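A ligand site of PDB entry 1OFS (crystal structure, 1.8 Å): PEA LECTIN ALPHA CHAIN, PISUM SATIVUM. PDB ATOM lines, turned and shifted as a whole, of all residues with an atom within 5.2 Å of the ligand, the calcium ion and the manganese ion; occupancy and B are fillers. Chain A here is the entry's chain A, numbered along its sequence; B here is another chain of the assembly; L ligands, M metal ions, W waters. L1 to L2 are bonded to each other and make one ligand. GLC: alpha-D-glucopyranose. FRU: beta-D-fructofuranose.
Four residues have an atom within 4 Å of the manganese ion: Glu 119, Asp 121, Asp 129 and His 136.
The nearest printed residue that does not touch the manganese ion is Ser 146 (4.2 Å).
An oxygen (O4) of GLC L1 sits at hydrogen-bond distance from the side-chain amide nitrogen (ND2) of Asn 125.
The side-chain carboxylate (OD2) of Asp 81 is in hydrogen-bond range of an oxygen (O4) of GLC L1 (2.5 Å).
An oxygen (O6) of GLC L1 sits at hydrogen-bond distance from the backbone NH (N) of Glu 31 of chain B (3.2 Å).
The backbone carbonyl oxygen (O) of Glu 31 of chain B is in hydrogen-bond range of an oxygen (O6) of GLC L1 (3.3 Å).
The side-chain carboxylate of Glu 31 of chain B sits at hydrogen-bond distance from an oxygen (O6) of FRU L2 (2.8 Å).
The backbone NH of Gly 99 lies within hydrogen-bond range of an oxygen (O3) of GLC L1 (2.9 Å).
O5 of GLC L1 sits at hydrogen-bond distance from N of Ala 30 of chain B (3.0 Å).
The backbone NH (N) of Gly 29 of chain B sits close to an oxygen (O6) of GLC L1.
The manganese ion is bound by OD2 of Asp 121 (2.1 Å), OD1 of Asp 129 (2.2 Å), OE1 of Glu 119 (2.2 Å), water W4 (2.3 Å) and NE2 of His 136 (2.3 Å).
CB of Ala 80 touches O6 of GLC L1, at 3.2 Å.
CA of Gly 98 touches O3 of GLC L1 (3.7 Å).
The nearest printed residue that does not touch the ligand is Thr 28 of chain B (4.5 Å).
The indole nitrogen (NE1) of Trp 128 sits close to the side-chain carboxylate (OD1) of Asp 129, 3.4 Å away.
The side-chain carboxylate (OE1) of Glu 119 lies close to the side-chain hydroxyl (OG) of Ser 146, at 3.5 Å.
The side-chain carboxylate (OD2) of Asp 81 lies close to the backbone NH (N) of Gly 99 (3.4 Å).
OD1 of Asp 81 is in hydrogen-bond range of N of Gly 29 of chain B (3.1 Å).
Water W5 lies within hydrogen-bond range of the backbone carbonyl oxygen (O) of Gly 99 (2.7 Å) and the indole nitrogen (NE1) of Trp 128 (3.0 Å).
Water W4 bridges OE2 of Glu 119 (2.6 Å) and O of Ile 144 (2.8 Å).
The side-chain amide oxygen (OD1) of Asn 125 binds the calcium ion, at 2.3 Å.
The calcium ion is bound by O of Phe 123.
OD2 of Asp 129 is bound to the calcium ion, 2.3 Å away.
OD1 of Asp 121 is bound to the calcium ion (2.4 Å).
Water W8 is bound to the calcium ion, 2.4 Å away.
OD2 of Asp 121 binds the calcium ion (2.4 Å).
Water W5 is bound to the calcium ion, at 2.5 Å.
The calcium ion has seven donor atoms within binding distance.
Within 4 Å of the calcium ion: Asp 121, Phe 123, Asn 125 and Asp 129.
Along chain A the residues within 4 Å of the calcium ion span positions 121 to 129.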
ATOM      1  N   ALA A  80     -17.939  -1.696  16.726  1.00  0.00           N
ATOM      2  CA  ALA A  80     -16.848  -2.607  16.398  1.00  0.00           C
ATOM      3  C   ALA A  80     -17.380  -3.674  15.461  1.00  0.00           C
ATOM      4  O   ALA A  80     -18.599  -3.822  15.340  1.00  0.00           O
ATOM      5  CB  ALA A  80     -16.260  -3.235  17.667  1.00  0.00           C
ATOM      6  N   ASP A  81     -16.507  -4.352  14.732  1.00  0.00           N
ATOM      7  CA  ASP A  81     -15.071  -4.094  14.764  1.00  0.00           C
ATOM      8  C   ASP A  81     -14.617  -3.478  13.454  1.00  0.00           C
ATOM      9  O   ASP A  81     -13.605  -2.794  13.388  1.00  0.00           O
ATOM     10  CB  ASP A  81     -14.285  -5.382  14.969  1.00  0.00           C
ATOM     11  CG  ASP A  81     -13.893  -5.577  16.407  1.00  0.00           C
ATOM     12  OD1 ASP A  81     -14.536  -6.408  17.077  1.00  0.00           O
ATOM     13  OD2 ASP A  81     -12.980  -4.926  16.940  1.00  0.00           O
ATOM     14  N   GLY A  97     -11.346 -13.444  14.506  1.00  0.00           N
ATOM     15  CA  GLY A  97     -12.400 -12.439  14.524  1.00  0.00           C
ATOM     16  C   GLY A  97     -12.085 -11.233  15.396  1.00  0.00           C
ATOM     17  O   GLY A  97     -10.915 -10.911  15.655  1.00  0.00           O
ATOM     18  N   GLY A  98     -13.130 -10.566  15.874  1.00  0.00           N
ATOM     19  CA  GLY A  98     -12.961  -9.383  16.689  1.00  0.00           C
ATOM     20  C   GLY A  98     -12.087  -8.363  15.978  1.00  0.00           C
ATOM     21  O   GLY A  98     -12.241  -8.100  14.774  1.00  0.00           O
ATOM     22  N   GLY A  99     -11.133  -7.802  16.721  1.00  0.00           N
ATOM     23  CA  GLY A  99     -10.225  -6.796  16.198  1.00  0.00           C
ATOM     24  C   GLY A  99      -9.329  -7.249  15.058  1.00  0.00           C
ATOM     25  O   GLY A  99      -8.680  -6.416  14.434  1.00  0.00           O
ATOM     26  N   TYR A 100      -9.273  -8.558  14.806  1.00  0.00           N
ATOM     27  CA  TYR A 100      -8.462  -9.095  13.713  1.00  0.00           C
ATOM     28  C   TYR A 100      -9.195  -9.107  12.369  1.00  0.00           C
ATOM     29  O   TYR A 100      -8.643  -9.510  11.354  1.00  0.00           O
ATOM     30  CB  TYR A 100      -7.902 -10.474  14.063  1.00  0.00           C
ATOM     31  CG  TYR A 100      -6.901 -10.419  15.203  1.00  0.00           C
ATOM     32  CD1 TYR A 100      -7.303 -10.634  16.516  1.00  0.00           C
ATOM     33  CD2 TYR A 100      -5.560 -10.121  14.968  1.00  0.00           C
ATOM     34  CE1 TYR A 100      -6.396 -10.579  17.564  1.00  0.00           C
ATOM     35  CE2 TYR A 100      -4.644 -10.052  16.010  1.00  0.00           C
ATOM     36  CZ  TYR A 100      -5.070 -10.295  17.306  1.00  0.00           C
ATOM     37  OH  TYR A 100      -4.184 -10.230  18.359  1.00  0.00           O
ATOM     38  N   GLU A 119      -8.748  -2.069   5.322  1.00  0.00           N
ATOM     39  CA  GLU A 119      -9.671  -2.069   6.452  1.00  0.00           C
ATOM     40  C   GLU A 119     -10.366  -0.746   6.724  1.00  0.00           C
ATOM     41  O   GLU A 119      -9.828   0.326   6.451  1.00  0.00           O
ATOM     42  CB  GLU A 119      -8.933  -2.493   7.740  1.00  0.00           C
ATOM     43  CG  GLU A 119      -7.844  -1.510   8.182  1.00  0.00           C
ATOM     44  CD  GLU A 119      -7.305  -1.823   9.570  1.00  0.00           C
ATOM     45  OE1 GLU A 119      -7.231  -0.910  10.407  1.00  0.00           O
ATOM     46  OE2 GLU A 119      -6.960  -3.002   9.828  1.00  0.00           O
ATOM     47  N   ASP A 121     -11.755   0.248   9.928  1.00  0.00           N
ATOM     48  CA  ASP A 121     -11.666  -0.099  11.342  1.00  0.00           C
ATOM     49  C   ASP A 121     -12.438   0.844  12.246  1.00  0.00           C
ATOM     50  O   ASP A 121     -12.078   2.006  12.370  1.00  0.00           O
ATOM     51  CB  ASP A 121     -10.160  -0.091  11.693  1.00  0.00           C
ATOM     52  CG  ASP A 121      -9.853  -0.793  12.982  1.00  0.00           C
ATOM     53  OD1 ASP A 121     -10.774  -0.959  13.803  1.00  0.00           O
ATOM     54  OD2 ASP A 121      -8.689  -1.192  13.287  1.00  0.00           O
ATOM     55  N   PHE A 123     -13.086   0.278  15.680  1.00  0.00           N
ATOM     56  CA  PHE A 123     -12.789   0.131  17.110  1.00  0.00           C
ATOM     57  C   PHE A 123     -11.298   0.201  17.410  1.00  0.00           C
ATOM     58  O   PHE A 123     -10.482  -0.461  16.776  1.00  0.00           O
ATOM     59  CB  PHE A 123     -13.381  -1.194  17.621  1.00  0.00           C
ATOM     60  CG  PHE A 123     -13.104  -1.459  19.074  1.00  0.00           C
ATOM     61  CD1 PHE A 123     -13.967  -1.002  20.059  1.00  0.00           C
ATOM     62  CD2 PHE A 123     -11.976  -2.170  19.465  1.00  0.00           C
ATOM     63  CE1 PHE A 123     -13.713  -1.251  21.400  1.00  0.00           C
ATOM     64  CE2 PHE A 123     -11.718  -2.426  20.795  1.00  0.00           C
ATOM     65  CZ  PHE A 123     -12.588  -1.970  21.769  1.00  0.00           C
ATOM     66  N   TYR A 124     -10.938   0.992  18.419  1.00  0.00           N
ATOM     67  CA  TYR A 124      -9.531   1.149  18.797  1.00  0.00           C
ATOM     68  C   TYR A 124      -8.981  -0.035  19.587  1.00  0.00           C
ATOM     69  O   TYR A 124      -9.379  -0.266  20.739  1.00  0.00           O
ATOM     70  CB  TYR A 124      -9.325   2.450  19.595  1.00  0.00           C
ATOM     71  CG  TYR A 124      -7.969   2.570  20.274  1.00  0.00           C
ATOM     72  CD1 TYR A 124      -6.798   2.646  19.522  1.00  0.00           C
ATOM     73  CD2 TYR A 124      -7.865   2.624  21.648  1.00  0.00           C
ATOM     74  CE1 TYR A 124      -5.558   2.764  20.148  1.00  0.00           C
ATOM     75  CE2 TYR A 124      -6.634   2.743  22.280  1.00  0.00           C
ATOM     76  CZ  TYR A 124      -5.492   2.813  21.521  1.00  0.00           C
ATOM     77  OH  TYR A 124      -4.260   2.932  22.153  1.00  0.00           O
ATOM     78  N   ASN A 125      -8.077  -0.779  18.973  1.00  0.00           N
ATOM     79  CA  ASN A 125      -7.401  -1.894  19.615  1.00  0.00           C
ATOM     80  C   ASN A 125      -6.047  -1.314  20.012  1.00  0.00           C
ATOM     81  O   ASN A 125      -5.168  -1.125  19.176  1.00  0.00           O
ATOM     82  CB  ASN A 125      -7.234  -3.079  18.655  1.00  0.00           C
ATOM     83  CG  ASN A 125      -8.550  -3.738  18.293  1.00  0.00           C
ATOM     84  OD1 ASN A 125      -9.134  -3.459  17.252  1.00  0.00           O
ATOM     85  ND2 ASN A 125      -9.023  -4.632  19.166  1.00  0.00           N
ATOM     86  N   TRP A 128      -2.314  -2.240  18.737  1.00  0.00           N
ATOM     87  CA  TRP A 128      -1.768  -1.934  17.431  1.00  0.00           C
ATOM     88  C   TRP A 128      -2.381  -0.782  16.640  1.00  0.00           C
ATOM     89  O   TRP A 128      -1.757  -0.283  15.710  1.00  0.00           O
ATOM     90  CB  TRP A 128      -1.800  -3.200  16.565  1.00  0.00           C
ATOM     91  CG  TRP A 128      -3.191  -3.698  16.340  1.00  0.00           C
ATOM     92  CD1 TRP A 128      -4.130  -3.158  15.505  1.00  0.00           C
ATOM     93  CD2 TRP A 128      -3.796  -4.824  16.966  1.00  0.00           C
ATOM     94  NE1 TRP A 128      -5.292  -3.888  15.583  1.00  0.00           N
ATOM     95  CE2 TRP A 128      -5.123  -4.916  16.461  1.00  0.00           C
ATOM     96  CE3 TRP A 128      -3.363  -5.781  17.893  1.00  0.00           C
ATOM     97  CZ2 TRP A 128      -6.000  -5.916  16.863  1.00  0.00           C
ATOM     98  CZ3 TRP A 128      -4.242  -6.760  18.289  1.00  0.00           C
ATOM     99  CH2 TRP A 128      -5.547  -6.832  17.778  1.00  0.00           C
ATOM    100  N   ASP A 129      -3.606  -0.365  16.985  1.00  0.00           N
ATOM    101  CA  ASP A 129      -4.259   0.708  16.237  1.00  0.00           C
ATOM    102  C   ASP A 129      -3.648   2.089  16.517  1.00  0.00           C
ATOM    103  O   ASP A 129      -2.966   2.263  17.530  1.00  0.00           O
ATOM    104  CB  ASP A 129      -5.772   0.720  16.510  1.00  0.00           C
ATOM    105  CG  ASP A 129      -6.520  -0.347  15.718  1.00  0.00           C
ATOM    106  OD1 ASP A 129      -6.064  -0.678  14.596  1.00  0.00           O
ATOM    107  OD2 ASP A 129      -7.547  -0.904  16.134  1.00  0.00           O
ATOM    108  N   PRO A 130      -3.866   3.040  15.612  1.00  0.00           N
ATOM    109  CA  PRO A 130      -3.317   4.390  15.781  1.00  0.00           C
ATOM    110  C   PRO A 130      -3.654   4.963  17.168  1.00  0.00           C
ATOM    111  O   PRO A 130      -4.798   4.911  17.601  1.00  0.00           O
ATOM    112  CB  PRO A 130      -4.005   5.183  14.666  1.00  0.00           C
ATOM    113  CG  PRO A 130      -4.251   4.148  13.613  1.00  0.00           C
ATOM    114  CD  PRO A 130      -4.633   2.900  14.367  1.00  0.00           C
ATOM    115  N   HIS A 136     -10.528   4.432  11.571  1.00  0.00           N
ATOM    116  CA  HIS A 136      -9.622   4.719  10.481  1.00  0.00           C
ATOM    117  C   HIS A 136      -9.653   3.715   9.350  1.00  0.00           C
ATOM    118  O   HIS A 136     -10.104   2.582   9.509  1.00  0.00           O
ATOM    119  CB  HIS A 136      -8.192   4.679  11.039  1.00  0.00           C
ATOM    120  CG  HIS A 136      -7.896   3.433  11.832  1.00  0.00           C
ATOM    121  ND1 HIS A 136      -8.244   3.300  13.160  1.00  0.00           N
ATOM    122  CD2 HIS A 136      -7.314   2.262  11.470  1.00  0.00           C
ATOM    123  CE1 HIS A 136      -7.889   2.109  13.588  1.00  0.00           C
ATOM    124  NE2 HIS A 136      -7.319   1.450  12.582  1.00  0.00           N
ATOM    125  N   ILE A 144      -2.420  -7.308  11.161  1.00  0.00           N
ATOM    126  CA  ILE A 144      -3.522  -6.409  11.512  1.00  0.00           C
ATOM    127  C   ILE A 144      -3.014  -4.998  11.832  1.00  0.00           C
ATOM    128  O   ILE A 144      -3.785  -4.037  11.890  1.00  0.00           O
ATOM    129  CB  ILE A 144      -4.347  -7.003  12.664  1.00  0.00           C
ATOM    130  CG1 ILE A 144      -5.691  -6.277  12.812  1.00  0.00           C
ATOM    131  CG2 ILE A 144      -3.545  -6.970  13.964  1.00  0.00           C
ATOM    132  CD1 ILE A 144      -6.648  -6.513  11.655  1.00  0.00           C
ATOM    133  N   SER A 146      -1.665  -2.050  10.483  1.00  0.00           N
ATOM    134  CA  SER A 146      -1.537  -1.427   9.163  1.00  0.00           C
ATOM    135  C   SER A 146      -0.198  -0.757   8.848  1.00  0.00           C
ATOM    136  O   SER A 146       0.468  -0.226   9.741  1.00  0.00           O
ATOM    137  CB  SER A 146      -2.660  -0.402   8.956  1.00  0.00           C
ATOM    138  OG  SER A 146      -3.907  -0.854   9.477  1.00  0.00           O
ATOM    139  N   THR B  28     -17.295  -8.587  14.596  1.00  0.00           N
ATOM    140  CA  THR B  28     -17.713  -7.892  15.797  1.00  0.00           C
ATOM    141  C   THR B  28     -17.006  -8.644  16.900  1.00  0.00           C
ATOM    142  O   THR B  28     -16.466  -9.734  16.665  1.00  0.00           O
ATOM    143  CB  THR B  28     -19.244  -7.918  15.991  1.00  0.00           C
ATOM    144  OG1 THR B  28     -19.721  -9.263  16.010  1.00  0.00           O
ATOM    145  CG2 THR B  28     -19.979  -7.298  14.790  1.00  0.00           C
ATOM    146  N   GLY B  29     -16.963  -8.063  18.096  1.00  0.00           N
ATOM    147  CA  GLY B  29     -16.336  -8.687  19.240  1.00  0.00           C
ATOM    148  C   GLY B  29     -17.244  -8.436  20.432  1.00  0.00           C
ATOM    149  O   GLY B  29     -18.422  -8.782  20.388  1.00  0.00           O
ATOM    150  N   ALA B  30     -16.708  -7.824  21.482  1.00  0.00           N
ATOM    151  CA  ALA B  30     -17.536  -7.494  22.656  1.00  0.00           C
ATOM    152  C   ALA B  30     -18.440  -6.313  22.301  1.00  0.00           C
ATOM    153  O   ALA B  30     -19.485  -6.098  22.944  1.00  0.00           O
ATOM    154  CB  ALA B  30     -16.674  -7.179  23.855  1.00  0.00           C
ATOM    155  N   GLU B  31     -18.033  -5.535  21.303  1.00  0.00           N
ATOM    156  CA  GLU B  31     -18.806  -4.405  20.806  1.00  0.00           C
ATOM    157  C   GLU B  31     -19.208  -4.812  19.392  1.00  0.00           C
ATOM    158  O   GLU B  31     -18.513  -5.628  18.778  1.00  0.00           O
ATOM    159  CB  GLU B  31     -18.028  -3.097  20.856  1.00  0.00           C
ATOM    160  CG  GLU B  31     -17.437  -2.770  22.226  1.00  0.00           C
ATOM    161  CD  GLU B  31     -18.494  -2.608  23.289  1.00  0.00           C
ATOM    162  OE1 GLU B  31     -19.675  -2.396  22.929  1.00  0.00           O
ATOM    163  OE2 GLU B  31     -18.145  -2.693  24.492  1.00  0.00           O
HETATM  164  C1  GLC L   1     -13.046  -7.591  22.522  1.00  0.00           C
HETATM  165  C2  GLC L   1     -12.289  -8.434  21.484  1.00  0.00           C
HETATM  166  C3  GLC L   1     -11.510  -7.515  20.508  1.00  0.00           C
HETATM  167  C4  GLC L   1     -12.497  -6.552  19.831  1.00  0.00           C
HETATM  168  C5  GLC L   1     -13.259  -5.748  20.923  1.00  0.00           C
HETATM  169  C6  GLC L   1     -14.346  -4.812  20.411  1.00  0.00           C
HETATM  170  O2  GLC L   1     -11.385  -9.279  22.144  1.00  0.00           O
HETATM  171  O3  GLC L   1     -10.899  -8.339  19.520  1.00  0.00           O
HETATM  172  O4  GLC L   1     -11.776  -5.635  19.009  1.00  0.00           O
HETATM  173  O5  GLC L   1     -13.954  -6.705  21.813  1.00  0.00           O
HETATM  174  O6  GLC L   1     -15.287  -5.588  19.645  1.00  0.00           O
HETATM  175  C1  FRU L   2     -12.257  -8.148  25.337  1.00  0.00           C
HETATM  176  C2  FRU L   2     -12.397  -6.776  24.695  1.00  0.00           C
HETATM  177  C3  FRU L   2     -11.455  -5.743  25.347  1.00  0.00           C
HETATM  178  C4  FRU L   2     -12.102  -4.471  24.878  1.00  0.00           C
HETATM  179  C5  FRU L   2     -13.563  -4.820  25.232  1.00  0.00           C
HETATM  180  C6  FRU L   2     -14.574  -4.010  24.447  1.00  0.00           C
HETATM  181  O1  FRU L   2     -12.690  -8.095  26.708  1.00  0.00           O
HETATM  182  O2  FRU L   2     -12.120  -6.863  23.289  1.00  0.00           O
HETATM  183  O3  FRU L   2     -10.132  -5.856  24.828  1.00  0.00           O
HETATM  184  O4  FRU L   2     -11.652  -3.358  25.658  1.00  0.00           O
HETATM  185  O5  FRU L   2     -13.699  -6.247  24.919  1.00  0.00           O
HETATM  186  O6  FRU L   2     -15.828  -4.102  25.068  1.00  0.00           O
HETATM  187 CA    CA M   1      -9.452  -2.062  15.425  1.00  0.00          CA
HETATM  188 MN    MN M   2      -6.761  -0.766  12.552  1.00  0.00          MN
HETATM  189  O   HOH W   1     -15.389  -8.530  27.145  1.00  0.00           O
HETATM  190  O   HOH W   2     -12.737  -3.283  28.229  1.00  0.00           O
HETATM  191  O   HOH W   3      -9.102  -8.046  23.493  1.00  0.00           O
HETATM  192  O   HOH W   4      -6.285  -2.967  12.314  1.00  0.00           O
HETATM  193  O   HOH W   5      -8.088  -3.810  14.382  1.00  0.00           O
HETATM  194  O   HOH W   6      -9.197  -4.315  22.706  1.00  0.00           O
HETATM  195  O   HOH W   7      -8.360  -4.858  26.739  1.00  0.00           O
HETATM  196  O   HOH W   8     -11.387  -3.438  15.248  1.00  0.00           O
HETATM  197  O   HOH W   9     -16.189  -5.875  27.139  1.00  0.00           O
HETATM  198  O   HOH W  10     -12.283  -0.566  24.847  1.00  0.00           O
HETATM  199  O   HOH W  11      -9.338 -10.751  20.053  1.00  0.00           O
